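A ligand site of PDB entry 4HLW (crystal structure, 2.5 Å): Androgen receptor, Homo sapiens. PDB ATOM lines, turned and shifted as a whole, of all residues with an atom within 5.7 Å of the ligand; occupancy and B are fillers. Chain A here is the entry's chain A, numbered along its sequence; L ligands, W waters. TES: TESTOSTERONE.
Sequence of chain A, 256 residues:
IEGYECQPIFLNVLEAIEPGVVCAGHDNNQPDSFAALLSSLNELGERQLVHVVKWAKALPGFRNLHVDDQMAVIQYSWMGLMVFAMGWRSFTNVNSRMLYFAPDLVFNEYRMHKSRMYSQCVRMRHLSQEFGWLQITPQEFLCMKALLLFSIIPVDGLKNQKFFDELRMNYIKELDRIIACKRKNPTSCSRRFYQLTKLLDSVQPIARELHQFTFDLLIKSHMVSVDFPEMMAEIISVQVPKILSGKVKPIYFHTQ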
ATOM      1  N   LEU A  38      15.190 -22.660  -6.543  1.00  0.00           N
ATOM      2  CA  LEU A  38      13.743 -22.587  -6.746  1.00  0.00           C
ATOM      3  C   LEU A  38      13.195 -23.638  -7.723  1.00  0.00           C
ATOM      4  O   LEU A  38      12.088 -24.151  -7.535  1.00  0.00           O
ATOM      5  CB  LEU A  38      13.307 -21.164  -7.134  1.00  0.00           C
ATOM      6  CG  LEU A  38      12.826 -20.315  -5.963  1.00  0.00           C
ATOM      7  CD1 LEU A  38      11.607 -20.920  -5.362  1.00  0.00           C
ATOM      8  CD2 LEU A  38      13.890 -20.194  -4.914  1.00  0.00           C
ATOM      9  N   LEU A  41      12.911 -26.838  -5.772  1.00  0.00           N
ATOM     10  CA  LEU A  41      11.694 -26.809  -4.947  1.00  0.00           C
ATOM     11  C   LEU A  41      10.477 -27.148  -5.799  1.00  0.00           C
ATOM     12  O   LEU A  41       9.671 -27.969  -5.420  1.00  0.00           O
ATOM     13  CB  LEU A  41      11.511 -25.458  -4.261  1.00  0.00           C
ATOM     14  CG  LEU A  41      12.414 -25.213  -3.050  1.00  0.00           C
ATOM     15  CD1 LEU A  41      12.256 -23.806  -2.483  1.00  0.00           C
ATOM     16  CD2 LEU A  41      12.135 -26.258  -1.970  1.00  0.00           C
ATOM     17  N   ASN A  42      10.380 -26.543  -6.978  1.00  0.00           N
ATOM     18  CA  ASN A  42       9.323 -26.841  -7.927  1.00  0.00           C
ATOM     19  C   ASN A  42       9.271 -28.314  -8.315  1.00  0.00           C
ATOM     20  O   ASN A  42       8.191 -28.923  -8.354  1.00  0.00           O
ATOM     21  CB  ASN A  42       9.464 -25.960  -9.174  1.00  0.00           C
ATOM     22  CG  ASN A  42       9.130 -24.520  -8.898  1.00  0.00           C
ATOM     23  OD1 ASN A  42       8.369 -24.214  -7.985  1.00  0.00           O
ATOM     24  ND2 ASN A  42       9.705 -23.611  -9.683  1.00  0.00           N
ATOM     25  N   LEU A  44      10.575 -30.792  -6.522  1.00  0.00           N
ATOM     26  CA  LEU A  44      10.208 -31.486  -5.290  1.00  0.00           C
ATOM     27  C   LEU A  44       8.709 -31.439  -5.107  1.00  0.00           C
ATOM     28  O   LEU A  44       8.079 -32.445  -4.777  1.00  0.00           O
ATOM     29  CB  LEU A  44      10.867 -30.837  -4.059  1.00  0.00           C
ATOM     30  CG  LEU A  44      10.595 -31.618  -2.766  1.00  0.00           C
ATOM     31  CD1 LEU A  44      11.134 -33.050  -2.887  1.00  0.00           C
ATOM     32  CD2 LEU A  44      11.177 -30.939  -1.525  1.00  0.00           C
ATOM     33  N   GLY A  45       8.156 -30.254  -5.333  1.00  0.00           N
ATOM     34  CA  GLY A  45       6.745 -29.997  -5.208  1.00  0.00           C
ATOM     35  C   GLY A  45       5.971 -30.938  -6.106  1.00  0.00           C
ATOM     36  O   GLY A  45       5.053 -31.609  -5.647  1.00  0.00           O
ATOM     37  N   GLN A  48       6.412 -34.510  -4.635  1.00  0.00           N
ATOM     38  CA  GLN A  48       5.637 -34.721  -3.427  1.00  0.00           C
ATOM     39  C   GLN A  48       4.147 -34.738  -3.689  1.00  0.00           C
ATOM     40  O   GLN A  48       3.377 -35.280  -2.915  1.00  0.00           O
ATOM     41  CB  GLN A  48       5.967 -33.656  -2.386  1.00  0.00           C
ATOM     42  CG  GLN A  48       7.075 -34.059  -1.443  1.00  0.00           C
ATOM     43  CD  GLN A  48       7.239 -33.043  -0.346  1.00  0.00           C
ATOM     44  OE1 GLN A  48       6.270 -32.430   0.099  1.00  0.00           O
ATOM     45  NE2 GLN A  48       8.474 -32.833   0.092  1.00  0.00           N
ATOM     46  N   TRP A  78      -2.518 -28.682  -0.758  1.00  0.00           N
ATOM     47  CA  TRP A  78      -1.162 -29.210  -0.845  1.00  0.00           C
ATOM     48  C   TRP A  78      -0.073 -28.330  -0.189  1.00  0.00           C
ATOM     49  O   TRP A  78       0.844 -28.848   0.454  1.00  0.00           O
ATOM     50  CB  TRP A  78      -0.812 -29.534  -2.302  1.00  0.00           C
ATOM     51  CG  TRP A  78      -0.913 -28.341  -3.168  1.00  0.00           C
ATOM     52  CD1 TRP A  78      -2.041 -27.850  -3.761  1.00  0.00           C
ATOM     53  CD2 TRP A  78       0.144 -27.450  -3.501  1.00  0.00           C
ATOM     54  NE1 TRP A  78      -1.745 -26.706  -4.460  1.00  0.00           N
ATOM     55  CE2 TRP A  78      -0.406 -26.437  -4.319  1.00  0.00           C
ATOM     56  CE3 TRP A  78       1.505 -27.407  -3.201  1.00  0.00           C
ATOM     57  CZ2 TRP A  78       0.359 -25.400  -4.837  1.00  0.00           C
ATOM     58  CZ3 TRP A  78       2.272 -26.379  -3.717  1.00  0.00           C
ATOM     59  CH2 TRP A  78       1.695 -25.390  -4.523  1.00  0.00           C
ATOM     60  N   MET A  79      -0.173 -27.024  -0.333  1.00  0.00           N
ATOM     61  CA  MET A  79       0.826 -26.138   0.265  1.00  0.00           C
ATOM     62  C   MET A  79       0.881 -26.344   1.773  1.00  0.00           C
ATOM     63  O   MET A  79       1.941 -26.615   2.336  1.00  0.00           O
ATOM     64  CB  MET A  79       0.523 -24.672  -0.070  1.00  0.00           C
ATOM     65  CG  MET A  79       1.572 -23.689   0.384  1.00  0.00           C
ATOM     66  SD  MET A  79       3.165 -23.958  -0.407  1.00  0.00           S
ATOM     67  CE  MET A  79       2.942 -23.123  -1.986  1.00  0.00           C
ATOM     68  N   MET A  82       2.179 -29.961   2.621  1.00  0.00           N
ATOM     69  CA  MET A  82       3.597 -30.113   2.388  1.00  0.00           C
ATOM     70  C   MET A  82       4.448 -29.275   3.328  1.00  0.00           C
ATOM     71  O   MET A  82       5.541 -29.687   3.693  1.00  0.00           O
ATOM     72  CB  MET A  82       3.912 -29.771   0.944  1.00  0.00           C
ATOM     73  CG  MET A  82       3.288 -30.746   0.001  1.00  0.00           C
ATOM     74  SD  MET A  82       3.657 -30.313  -1.677  1.00  0.00           S
ATOM     75  CE  MET A  82       2.869 -31.643  -2.555  1.00  0.00           C
ATOM     76  N   VAL A  83       3.936 -28.129   3.740  1.00  0.00           N
ATOM     77  CA  VAL A  83       4.662 -27.272   4.669  1.00  0.00           C
ATOM     78  C   VAL A  83       4.650 -27.826   6.075  1.00  0.00           C
ATOM     79  O   VAL A  83       5.656 -27.816   6.772  1.00  0.00           O
ATOM     80  CB  VAL A  83       4.072 -25.870   4.669  1.00  0.00           C
ATOM     81  CG1 VAL A  83       4.419 -25.132   5.945  1.00  0.00           C
ATOM     82  CG2 VAL A  83       4.579 -25.116   3.467  1.00  0.00           C
ATOM     83  N   MET A  86       6.983 -30.797   6.201  1.00  0.00           N
ATOM     84  CA  MET A  86       8.377 -30.381   6.120  1.00  0.00           C
ATOM     85  C   MET A  86       8.889 -29.917   7.492  1.00  0.00           C
ATOM     86  O   MET A  86       9.966 -30.318   7.945  1.00  0.00           O
ATOM     87  CB  MET A  86       8.536 -29.294   5.044  1.00  0.00           C
ATOM     88  CG  MET A  86       9.962 -28.844   4.777  1.00  0.00           C
ATOM     89  SD  MET A  86      10.450 -27.470   5.840  1.00  0.00           S
ATOM     90  CE  MET A  86       9.463 -26.138   5.155  1.00  0.00           C
ATOM     91  N   ARG A  89       9.636 -32.906   9.430  1.00  0.00           N
ATOM     92  CA  ARG A  89      10.924 -33.498   9.034  1.00  0.00           C
ATOM     93  C   ARG A  89      12.049 -32.693   9.633  1.00  0.00           C
ATOM     94  O   ARG A  89      12.975 -33.250  10.222  1.00  0.00           O
ATOM     95  CB  ARG A  89      11.124 -33.529   7.510  1.00  0.00           C
ATOM     96  CG  ARG A  89      10.216 -34.488   6.758  1.00  0.00           C
ATOM     97  CD  ARG A  89      10.641 -34.657   5.292  1.00  0.00           C
ATOM     98  NE  ARG A  89      10.631 -33.427   4.497  1.00  0.00           N
ATOM     99  CZ  ARG A  89       9.550 -32.916   3.914  1.00  0.00           C
ATOM    100  NH1 ARG A  89       8.370 -33.515   4.030  1.00  0.00           N
ATOM    101  NH2 ARG A  89       9.659 -31.796   3.196  1.00  0.00           N
ATOM    102  N   PHE A 101      13.778 -29.795   3.466  1.00  0.00           N
ATOM    103  CA  PHE A 101      12.797 -30.035   2.422  1.00  0.00           C
ATOM    104  C   PHE A 101      12.883 -31.449   1.881  1.00  0.00           C
ATOM    105  O   PHE A 101      11.879 -32.076   1.546  1.00  0.00           O
ATOM    106  CB  PHE A 101      12.971 -29.025   1.299  1.00  0.00           C
ATOM    107  CG  PHE A 101      12.642 -27.638   1.675  1.00  0.00           C
ATOM    108  CD1 PHE A 101      11.326 -27.201   1.677  1.00  0.00           C
ATOM    109  CD2 PHE A 101      13.630 -26.751   2.048  1.00  0.00           C
ATOM    110  CE1 PHE A 101      11.015 -25.908   2.028  1.00  0.00           C
ATOM    111  CE2 PHE A 101      13.307 -25.448   2.408  1.00  0.00           C
ATOM    112  CZ  PHE A 101      11.984 -25.025   2.391  1.00  0.00           C
ATOM    113  N   MET A 117      13.546 -16.017  -0.223  1.00  0.00           N
ATOM    114  CA  MET A 117      12.357 -16.420   0.510  1.00  0.00           C
ATOM    115  C   MET A 117      12.583 -16.323   2.002  1.00  0.00           C
ATOM    116  O   MET A 117      11.897 -16.997   2.763  1.00  0.00           O
ATOM    117  CB  MET A 117      12.032 -17.869   0.231  1.00  0.00           C
ATOM    118  CG  MET A 117      11.472 -18.130  -1.106  1.00  0.00           C
ATOM    119  SD  MET A 117      10.286 -19.456  -0.966  1.00  0.00           S
ATOM    120  CE  MET A 117      11.367 -20.775  -0.418  1.00  0.00           C
ATOM    121  N   MET A 124       8.368 -20.593   8.480  1.00  0.00           N
ATOM    122  CA  MET A 124       8.391 -22.042   8.398  1.00  0.00           C
ATOM    123  C   MET A 124       9.264 -22.647   9.478  1.00  0.00           C
ATOM    124  O   MET A 124       8.937 -23.697  10.038  1.00  0.00           O
ATOM    125  CB  MET A 124       8.863 -22.498   7.011  1.00  0.00           C
ATOM    126  CG  MET A 124       7.954 -22.036   5.910  1.00  0.00           C
ATOM    127  SD  MET A 124       8.213 -22.923   4.374  1.00  0.00           S
ATOM    128  CE  MET A 124       9.407 -21.887   3.551  1.00  0.00           C
ATOM    129  N   LEU A 210       3.074 -18.364   1.011  1.00  0.00           N
ATOM    130  CA  LEU A 210       3.723 -19.167   0.006  1.00  0.00           C
ATOM    131  C   LEU A 210       2.931 -19.152  -1.299  1.00  0.00           C
ATOM    132  O   LEU A 210       3.515 -19.102  -2.363  1.00  0.00           O
ATOM    133  CB  LEU A 210       3.987 -20.565   0.531  1.00  0.00           C
ATOM    134  CG  LEU A 210       5.032 -20.589   1.652  1.00  0.00           C
ATOM    135  CD1 LEU A 210       5.082 -21.920   2.365  1.00  0.00           C
ATOM    136  CD2 LEU A 210       6.420 -20.211   1.120  1.00  0.00           C
ATOM    137  N   PHE A 213       3.797 -15.878  -2.907  1.00  0.00           N
ATOM    138  CA  PHE A 213       5.157 -15.915  -3.437  1.00  0.00           C
ATOM    139  C   PHE A 213       5.291 -16.730  -4.729  1.00  0.00           C
ATOM    140  O   PHE A 213       5.816 -16.245  -5.714  1.00  0.00           O
ATOM    141  CB  PHE A 213       6.111 -16.449  -2.382  1.00  0.00           C
ATOM    142  CG  PHE A 213       7.547 -16.371  -2.793  1.00  0.00           C
ATOM    143  CD1 PHE A 213       8.303 -15.247  -2.493  1.00  0.00           C
ATOM    144  CD2 PHE A 213       8.145 -17.426  -3.477  1.00  0.00           C
ATOM    145  CE1 PHE A 213       9.626 -15.171  -2.861  1.00  0.00           C
ATOM    146  CE2 PHE A 213       9.459 -17.354  -3.865  1.00  0.00           C
ATOM    147  CZ  PHE A 213      10.204 -16.221  -3.557  1.00  0.00           C
ATOM    148  N   THR A 214       4.805 -17.968  -4.697  1.00  0.00           N
ATOM    149  CA  THR A 214       4.949 -18.876  -5.822  1.00  0.00           C
ATOM    150  C   THR A 214       4.195 -18.339  -7.055  1.00  0.00           C
ATOM    151  O   THR A 214       4.639 -18.519  -8.184  1.00  0.00           O
ATOM    152  CB  THR A 214       4.493 -20.308  -5.453  1.00  0.00           C
ATOM    153  OG1 THR A 214       4.787 -21.214  -6.527  1.00  0.00           O
ATOM    154  CG2 THR A 214       2.997 -20.364  -5.151  1.00  0.00           C
ATOM    155  N   LEU A 217       6.157 -15.599  -8.594  1.00  0.00           N
ATOM    156  CA  LEU A 217       7.296 -16.274  -9.210  1.00  0.00           C
ATOM    157  C   LEU A 217       6.914 -16.914 -10.535  1.00  0.00           C
ATOM    158  O   LEU A 217       7.656 -16.861 -11.497  1.00  0.00           O
ATOM    159  CB  LEU A 217       7.874 -17.308  -8.244  1.00  0.00           C
ATOM    160  CG  LEU A 217       9.009 -18.216  -8.772  1.00  0.00           C
ATOM    161  CD1 LEU A 217      10.112 -17.392  -9.426  1.00  0.00           C
ATOM    162  CD2 LEU A 217       9.583 -19.028  -7.650  1.00  0.00           C
ATOM    163  N   PHE A 228       9.022 -24.434 -14.014  1.00  0.00           N
ATOM    164  CA  PHE A 228       7.880 -25.043 -13.326  1.00  0.00           C
ATOM    165  C   PHE A 228       7.416 -26.272 -14.107  1.00  0.00           C
ATOM    166  O   PHE A 228       7.127 -26.196 -15.306  1.00  0.00           O
ATOM    167  CB  PHE A 228       6.718 -24.051 -13.240  1.00  0.00           C
ATOM    168  CG  PHE A 228       6.816 -23.078 -12.098  1.00  0.00           C
ATOM    169  CD1 PHE A 228       7.619 -21.952 -12.192  1.00  0.00           C
ATOM    170  CD2 PHE A 228       6.081 -23.272 -10.941  1.00  0.00           C
ATOM    171  CE1 PHE A 228       7.701 -21.041 -11.154  1.00  0.00           C
ATOM    172  CE2 PHE A 228       6.164 -22.369  -9.892  1.00  0.00           C
ATOM    173  CZ  PHE A 228       6.970 -21.256 -10.003  1.00  0.00           C
ATOM    174  N   MET A 232       2.574 -28.264 -11.445  1.00  0.00           N
ATOM    175  CA  MET A 232       2.737 -27.059 -10.631  1.00  0.00           C
ATOM    176  C   MET A 232       2.260 -25.832 -11.407  1.00  0.00           C
ATOM    177  O   MET A 232       1.459 -25.028 -10.910  1.00  0.00           O
ATOM    178  CB  MET A 232       4.183 -26.901 -10.160  1.00  0.00           C
ATOM    179  CG  MET A 232       4.651 -27.998  -9.213  1.00  0.00           C
ATOM    180  SD  MET A 232       4.024 -27.835  -7.526  1.00  0.00           S
ATOM    181  CE  MET A 232       4.848 -26.334  -7.007  1.00  0.00           C
ATOM    182  N   ILE A 236      -0.833 -23.629 -10.042  1.00  0.00           N
ATOM    183  CA  ILE A 236      -0.516 -22.295  -9.583  1.00  0.00           C
ATOM    184  C   ILE A 236      -1.221 -21.206 -10.404  1.00  0.00           C
ATOM    185  O   ILE A 236      -1.453 -20.111  -9.904  1.00  0.00           O
ATOM    186  CB  ILE A 236       0.990 -22.105  -9.469  1.00  0.00           C
ATOM    187  CG1 ILE A 236       1.478 -22.964  -8.294  1.00  0.00           C
ATOM    188  CG2 ILE A 236       1.366 -20.639  -9.260  1.00  0.00           C
ATOM    189  CD1 ILE A 236       2.960 -23.098  -8.180  1.00  0.00           C
HETATM  190  C1  TES L   1       7.837 -28.268  -1.815  1.00  0.00           C
HETATM  191  C2  TES L   1       7.545 -29.380  -0.876  1.00  0.00           C
HETATM  192  C3  TES L   1       7.922 -28.950   0.492  1.00  0.00           C
HETATM  193  O3  TES L   1       8.408 -29.765   1.264  1.00  0.00           O
HETATM  194  C4  TES L   1       7.687 -27.537   0.931  1.00  0.00           C
HETATM  195  C5  TES L   1       7.295 -26.587   0.012  1.00  0.00           C
HETATM  196  C6  TES L   1       7.050 -25.114   0.451  1.00  0.00           C
HETATM  197  C7  TES L   1       7.762 -24.234  -0.574  1.00  0.00           C
HETATM  198  C8  TES L   1       7.276 -24.555  -1.977  1.00  0.00           C
HETATM  199  C9  TES L   1       7.621 -25.984  -2.315  1.00  0.00           C
HETATM  200  C10 TES L   1       7.098 -26.961  -1.505  1.00  0.00           C
HETATM  201  C11 TES L   1       7.104 -26.185  -3.952  1.00  0.00           C
HETATM  202  C12 TES L   1       7.808 -24.945  -4.852  1.00  0.00           C
HETATM  203  C13 TES L   1       7.458 -23.726  -4.228  1.00  0.00           C
HETATM  204  C14 TES L   1       7.935 -23.687  -2.902  1.00  0.00           C
HETATM  205  C15 TES L   1       7.763 -22.164  -2.486  1.00  0.00           C
HETATM  206  C16 TES L   1       8.140 -21.426  -3.897  1.00  0.00           C
HETATM  207  C17 TES L   1       8.168 -22.571  -4.910  1.00  0.00           C
HETATM  208  O17 TES L   1       7.601 -22.188  -6.086  1.00  0.00           O
HETATM  209  C18 TES L   1       5.975 -23.481  -4.288  1.00  0.00           C
HETATM  210  C19 TES L   1       5.645 -27.195  -1.751  1.00  0.00           C
HETATM  211  O   HOH W   1       6.421 -32.076   2.570  1.00  0.00           O
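Residues that only touch the ligand: Leu 41, Met 82, Phe 101, Leu 38, Met 232, Met 86, Met 79, Val 83, Gly 45 and Trp 78.
Hydrophobic or aromatic side chains that line the ligand: Leu 38, Leu 41, Trp 78, Met 79, Met 82, Val 83, Met 86, Phe 101 and Met 232.
Of the 22 residues printed, 14 come within 4 Å of the ligand.
The side-chain amide nitrogen (ND2) of Asn 42 sits at hydrogen-bond distance from the backbone carbonyl oxygen (O) of Leu 38 (3.3 Å).
The guanidinium group of Arg 89 sits close to the side-chain amide nitrogen of Gln 48, 3.5 Å away.
The backbone carbonyl oxygen of Phe 101 sits at hydrogen-bond distance from the guanidinium group of Arg 89.
O17 of the ligand is in hydrogen-bond range of OD1 of Asn 42 (2.9 Å).
OG1 of Thr 214 lies within hydrogen-bond range of O17 of the ligand (3.0 Å).
The guanidinium group (NH2) of Arg 89 is in hydrogen-bond range of an oxygen (O3) of the ligand (3.1 Å).
NE2 of Gln 48 is in hydrogen-bond range of O3 of the ligand (3.3 Å).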
